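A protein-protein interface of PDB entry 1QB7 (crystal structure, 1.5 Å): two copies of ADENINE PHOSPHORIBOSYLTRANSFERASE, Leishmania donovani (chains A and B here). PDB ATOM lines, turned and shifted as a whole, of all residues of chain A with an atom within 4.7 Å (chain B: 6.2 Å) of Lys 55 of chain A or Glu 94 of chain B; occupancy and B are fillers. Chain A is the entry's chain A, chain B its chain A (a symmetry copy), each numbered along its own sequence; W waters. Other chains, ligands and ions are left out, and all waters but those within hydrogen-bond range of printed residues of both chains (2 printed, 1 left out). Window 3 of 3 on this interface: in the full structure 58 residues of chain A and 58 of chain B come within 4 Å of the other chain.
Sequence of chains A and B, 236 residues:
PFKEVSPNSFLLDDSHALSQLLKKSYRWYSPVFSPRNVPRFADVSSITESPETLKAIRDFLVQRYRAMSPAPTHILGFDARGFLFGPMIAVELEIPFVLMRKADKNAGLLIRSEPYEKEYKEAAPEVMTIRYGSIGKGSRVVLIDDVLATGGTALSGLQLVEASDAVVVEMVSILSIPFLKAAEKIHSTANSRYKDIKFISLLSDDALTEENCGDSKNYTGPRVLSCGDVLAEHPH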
ATOM      1  N   PRO A  51      19.253   1.312  12.951  1.00  0.00           N
ATOM      2  CA  PRO A  51      20.620   1.299  12.424  1.00  0.00           C
ATOM      3  C   PRO A  51      20.951   2.484  11.521  1.00  0.00           C
ATOM      4  O   PRO A  51      21.996   3.117  11.673  1.00  0.00           O
ATOM      5  CB  PRO A  51      20.667  -0.020  11.656  1.00  0.00           C
ATOM      6  CG  PRO A  51      19.780  -0.891  12.453  1.00  0.00           C
ATOM      7  CD  PRO A  51      18.604   0.006  12.732  1.00  0.00           C
ATOM      8  N   GLU A  52      20.045   2.798  10.602  1.00  0.00           N
ATOM      9  CA  GLU A  52      20.266   3.897   9.670  1.00  0.00           C
ATOM     10  C   GLU A  52      20.316   5.241  10.393  1.00  0.00           C
ATOM     11  O   GLU A  52      21.149   6.090  10.075  1.00  0.00           O
ATOM     12  CB  GLU A  52      19.181   3.909   8.587  1.00  0.00           C
ATOM     13  CG  GLU A  52      19.501   4.835   7.424  1.00  0.00           C
ATOM     14  CD  GLU A  52      18.356   5.002   6.434  1.00  0.00           C
ATOM     15  OE1 GLU A  52      17.225   4.531   6.707  1.00  0.00           O
ATOM     16  OE2 GLU A  52      18.592   5.631   5.377  1.00  0.00           O
ATOM     17  N   THR A  53      19.447   5.422  11.385  1.00  0.00           N
ATOM     18  CA  THR A  53      19.414   6.677  12.129  1.00  0.00           C
ATOM     19  C   THR A  53      20.653   6.841  13.006  1.00  0.00           C
ATOM     20  O   THR A  53      21.258   7.912  13.038  1.00  0.00           O
ATOM     21  CB  THR A  53      18.128   6.805  12.981  1.00  0.00           C
ATOM     22  OG1 THR A  53      16.986   6.530  12.162  1.00  0.00           O
ATOM     23  CG2 THR A  53      17.990   8.217  13.542  1.00  0.00           C
ATOM     24  N   LEU A  54      21.055   5.771  13.683  1.00  0.00           N
ATOM     25  CA  LEU A  54      22.229   5.825  14.547  1.00  0.00           C
ATOM     26  C   LEU A  54      23.470   6.170  13.712  1.00  0.00           C
ATOM     27  O   LEU A  54      24.275   7.027  14.096  1.00  0.00           O
ATOM     28  CB  LEU A  54      22.417   4.487  15.265  1.00  0.00           C
ATOM     29  CG  LEU A  54      23.349   4.462  16.476  1.00  0.00           C
ATOM     30  CD1 LEU A  54      22.827   5.366  17.592  1.00  0.00           C
ATOM     31  CD2 LEU A  54      23.458   3.034  16.965  1.00  0.00           C
ATOM     32  N   LYS A  55      23.585   5.542  12.543  1.00  0.00           N
ATOM     33  CA  LYS A  55      24.708   5.784  11.649  1.00  0.00           C
ATOM     34  C   LYS A  55      24.707   7.228  11.133  1.00  0.00           C
ATOM     35  O   LYS A  55      25.757   7.867  11.048  1.00  0.00           O
ATOM     36  CB  LYS A  55      24.679   4.798  10.478  1.00  0.00           C
ATOM     37  CG  LYS A  55      25.903   4.886   9.586  1.00  0.00           C
ATOM     38  CD  LYS A  55      25.832   3.918   8.429  1.00  0.00           C
ATOM     39  CE  LYS A  55      26.995   4.145   7.477  1.00  0.00           C
ATOM     40  NZ  LYS A  55      26.977   3.199   6.318  1.00  0.00           N
ATOM     41  N   ALA A  56      23.522   7.747  10.827  1.00  0.00           N
ATOM     42  CA  ALA A  56      23.391   9.116  10.333  1.00  0.00           C
ATOM     43  C   ALA A  56      23.872  10.123  11.377  1.00  0.00           C
ATOM     44  O   ALA A  56      24.540  11.102  11.039  1.00  0.00           O
ATOM     45  CB  ALA A  56      21.950   9.401   9.932  1.00  0.00           C
ATOM     46  N   ILE A  57      23.542   9.874  12.643  1.00  0.00           N
ATOM     47  CA  ILE A  57      23.957  10.747  13.742  1.00  0.00           C
ATOM     48  C   ILE A  57      25.475  10.679  13.884  1.00  0.00           C
ATOM     49  O   ILE A  57      26.149  11.704  13.972  1.00  0.00           O
ATOM     50  CB  ILE A  57      23.333  10.306  15.077  1.00  0.00           C
ATOM     51  CG1 ILE A  57      21.819  10.509  15.044  1.00  0.00           C
ATOM     52  CG2 ILE A  57      23.971  11.064  16.236  1.00  0.00           C
ATOM     53  CD1 ILE A  57      21.102   9.864  16.195  1.00  0.00           C
ATOM     54  N   ARG A  58      26.001   9.457  13.899  1.00  0.00           N
ATOM     55  CA  ARG A  58      27.436   9.227  14.027  1.00  0.00           C
ATOM     56  C   ARG A  58      28.197   9.934  12.899  1.00  0.00           C
ATOM     57  O   ARG A  58      29.137  10.687  13.154  1.00  0.00           O
ATOM     58  CB  ARG A  58      27.712   7.720  13.996  1.00  0.00           C
ATOM     59  CG  ARG A  58      29.106   7.298  14.417  1.00  0.00           C
ATOM     60  CD  ARG A  58      30.141   7.516  13.325  1.00  0.00           C
ATOM     61  NE  ARG A  58      29.739   6.907  12.060  1.00  0.00           N
ATOM     62  CZ  ARG A  58      29.892   5.621  11.749  1.00  0.00           C
ATOM     63  NH1 ARG A  58      30.454   4.780  12.610  1.00  0.00           N
ATOM     64  NH2 ARG A  58      29.487   5.175  10.566  1.00  0.00           N
ATOM     65  N   ASP A  59      27.773   9.703  11.660  1.00  0.00           N
ATOM     66  CA  ASP A  59      28.425  10.313  10.500  1.00  0.00           C
ATOM     67  C   ASP A  59      28.405  11.835  10.536  1.00  0.00           C
ATOM     68  O   ASP A  59      29.425  12.477  10.304  1.00  0.00           O
ATOM     69  CB  ASP A  59      27.777   9.837   9.193  1.00  0.00           C
ATOM     70  CG  ASP A  59      28.053   8.380   8.894  1.00  0.00           C
ATOM     71  OD1 ASP A  59      29.017   7.814   9.442  1.00  0.00           O
ATOM     72  OD2 ASP A  59      27.302   7.797   8.089  1.00  0.00           O
ATOM     73  N   ILE B  89      29.356  -0.815  18.164  1.00  0.00           N
ATOM     74  CA  ILE B  89      29.466  -2.087  17.459  1.00  0.00           C
ATOM     75  C   ILE B  89      28.249  -2.238  16.544  1.00  0.00           C
ATOM     76  O   ILE B  89      28.385  -2.514  15.350  1.00  0.00           O
ATOM     77  CB  ILE B  89      29.514  -3.270  18.440  1.00  0.00           C
ATOM     78  CG1 ILE B  89      30.763  -3.174  19.319  1.00  0.00           C
ATOM     79  CG2 ILE B  89      29.528  -4.588  17.682  1.00  0.00           C
ATOM     80  CD1 ILE B  89      30.733  -4.111  20.514  1.00  0.00           C
ATOM     81  N   ALA B  90      27.066  -2.011  17.114  1.00  0.00           N
ATOM     82  CA  ALA B  90      25.801  -2.114  16.395  1.00  0.00           C
ATOM     83  C   ALA B  90      25.723  -1.202  15.169  1.00  0.00           C
ATOM     84  O   ALA B  90      25.156  -1.585  14.143  1.00  0.00           O
ATOM     85  CB  ALA B  90      24.632  -1.828  17.342  1.00  0.00           C
ATOM     86  N   VAL B  91      26.304  -0.008  15.271  1.00  0.00           N
ATOM     87  CA  VAL B  91      26.293   0.948  14.162  1.00  0.00           C
ATOM     88  C   VAL B  91      27.069   0.407  12.955  1.00  0.00           C
ATOM     89  O   VAL B  91      26.694   0.645  11.806  1.00  0.00           O
ATOM     90  CB  VAL B  91      26.845   2.339  14.597  1.00  0.00           C
ATOM     91  CG1 VAL B  91      28.352   2.302  14.760  1.00  0.00           C
ATOM     92  CG2 VAL B  91      26.434   3.403  13.605  1.00  0.00           C
ATOM     93  N   GLU B  92      28.123  -0.357  13.228  1.00  0.00           N
ATOM     94  CA  GLU B  92      28.941  -0.950  12.178  1.00  0.00           C
ATOM     95  C   GLU B  92      28.273  -2.185  11.574  1.00  0.00           C
ATOM     96  O   GLU B  92      28.328  -2.407  10.363  1.00  0.00           O
ATOM     97  CB  GLU B  92      30.314  -1.329  12.734  1.00  0.00           C
ATOM     98  CG  GLU B  92      31.132  -0.148  13.222  1.00  0.00           C
ATOM     99  CD  GLU B  92      31.351   0.912  12.149  1.00  0.00           C
ATOM    100  OE1 GLU B  92      31.331   0.582  10.943  1.00  0.00           O
ATOM    101  OE2 GLU B  92      31.558   2.086  12.513  1.00  0.00           O
ATOM    102  N   LEU B  93      27.677  -3.003  12.436  1.00  0.00           N
ATOM    103  CA  LEU B  93      26.990  -4.217  12.017  1.00  0.00           C
ATOM    104  C   LEU B  93      25.645  -3.880  11.388  1.00  0.00           C
ATOM    105  O   LEU B  93      25.010  -4.734  10.762  1.00  0.00           O
ATOM    106  CB  LEU B  93      26.758  -5.134  13.220  1.00  0.00           C
ATOM    107  CG  LEU B  93      27.980  -5.668  13.963  1.00  0.00           C
ATOM    108  CD1 LEU B  93      27.525  -6.495  15.159  1.00  0.00           C
ATOM    109  CD2 LEU B  93      28.830  -6.494  13.019  1.00  0.00           C
ATOM    110  N   GLU B  94      25.205  -2.639  11.599  1.00  0.00           N
ATOM    111  CA  GLU B  94      23.933  -2.148  11.082  1.00  0.00           C
ATOM    112  C   GLU B  94      22.749  -2.954  11.618  1.00  0.00           C
ATOM    113  O   GLU B  94      21.866  -3.370  10.862  1.00  0.00           O
ATOM    114  CB  GLU B  94      23.946  -2.126   9.550  1.00  0.00           C
ATOM    115  CG  GLU B  94      25.045  -1.233   8.984  1.00  0.00           C
ATOM    116  CD  GLU B  94      25.067  -1.174   7.462  1.00  0.00           C
ATOM    117  OE1 GLU B  94      24.483  -2.067   6.808  1.00  0.00           O
ATOM    118  OE2 GLU B  94      25.680  -0.227   6.921  1.00  0.00           O
ATOM    119  N   ILE B  95      22.772  -3.213  12.927  1.00  0.00           N
ATOM    120  CA  ILE B  95      21.698  -3.939  13.605  1.00  0.00           C
ATOM    121  C   ILE B  95      21.250  -3.087  14.799  1.00  0.00           C
ATOM    122  O   ILE B  95      21.968  -2.179  15.229  1.00  0.00           O
ATOM    123  CB  ILE B  95      22.132  -5.366  14.070  1.00  0.00           C
ATOM    124  CG1 ILE B  95      23.342  -5.294  15.009  1.00  0.00           C
ATOM    125  CG2 ILE B  95      22.415  -6.255  12.857  1.00  0.00           C
ATOM    126  CD1 ILE B  95      23.768  -6.637  15.563  1.00  0.00           C
ATOM    127  N   PRO B  96      20.038  -3.338  15.318  1.00  0.00           N
ATOM    128  CA  PRO B  96      19.505  -2.578  16.455  1.00  0.00           C
ATOM    129  C   PRO B  96      20.284  -2.721  17.762  1.00  0.00           C
ATOM    130  O   PRO B  96      20.889  -3.767  18.029  1.00  0.00           O
ATOM    131  CB  PRO B  96      18.102  -3.178  16.637  1.00  0.00           C
ATOM    132  CG  PRO B  96      17.754  -3.681  15.292  1.00  0.00           C
ATOM    133  CD  PRO B  96      19.040  -4.307  14.836  1.00  0.00           C
HETATM  134  O   HOH W   1      30.101   2.545   9.332  1.00  0.00           O
HETATM  135  O   HOH W   2      24.205   1.349  11.037  1.00  0.00           O
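No position is printed for both chains.
The backbone carbonyl oxygen of Ala 90 of chain B lies within hydrogen-bond range of the backbone NH of Ile 95 of chain B, 3.1 Å away. NE of Arg 58 of chain A is in salt-bridge range of OD1 of Asp 59 of chain A.
Water W2 bridges the backbone carbonyl oxygen of Val 91 of chain B (2.7 Å) and the backbone carbonyl oxygen of Pro 51 of chain A (2.9 Å). Water W1 lies within hydrogen-bond range of OE1 of Glu 92 of chain B (2.8 Å) and NH2 of Arg 58 of chain A (3.0 Å).
Printed residues of chain B within 4 Å of Lys 55 of chain A: Val 91 (3.5 Å) and Glu 94 (3.7 Å). Of the printed residues of chain B, Arg 58 of chain A touches Val 91 (3.9 Å) and Glu 92 (2.9 Å). Of the printed residues of chain A, Glu 92 of chain B touches Arg 58 (2.9 Å). Of chain A, only Pro 51 and Lys 55 come within 4 Å of Glu 94 of chain B. Of the printed residues of chain A, Ile 95 of chain B touches Pro 51 (3.5 Å). Of the printed residues of chain A, Pro 96 of chain B touches Pro 51. The nearest printed residue of chain B that does not touch Lys 55 of chain A is Glu 92 of chain B (6.6 Å). The nearest printed residue of chain A that does not touch Glu 94 of chain B is Glu 52 of chain A (6.3 Å).
The side-chain amino group (NZ) of Lys 55 of chain A is in salt-bridge range of the side-chain carboxylate (OE2) of Glu 94 of chain B, 3.7 Å away. NH1 of Arg 58 of chain A lies within salt-bridge range of OE2 of Glu 92 of chain B (2.9 Å).
Pro 51 of chain A touches Glu 94 of chain B (CB to C, 3.6 Å). Ile 95 of chain B touches Pro 51 of chain A (C to CG, 3.5 Å). CG of Pro 51 of chain A touches N of Pro 96 of chain B (3.8 Å). CG2 of Val 91 of chain B touches CA of Lys 55 of chain A, at 3.5 Å. NH1 of Arg 58 of chain A touches CG1 of Val 91 of chain B, at 3.9 Å.
Printed residues of chain A that touch a printed residue of chain B: Pro 51, Lys 55 and Arg 58. Hydrophobic or aromatic side chains of chain A within 4 Å of the printed part of chain B: Pro 51.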
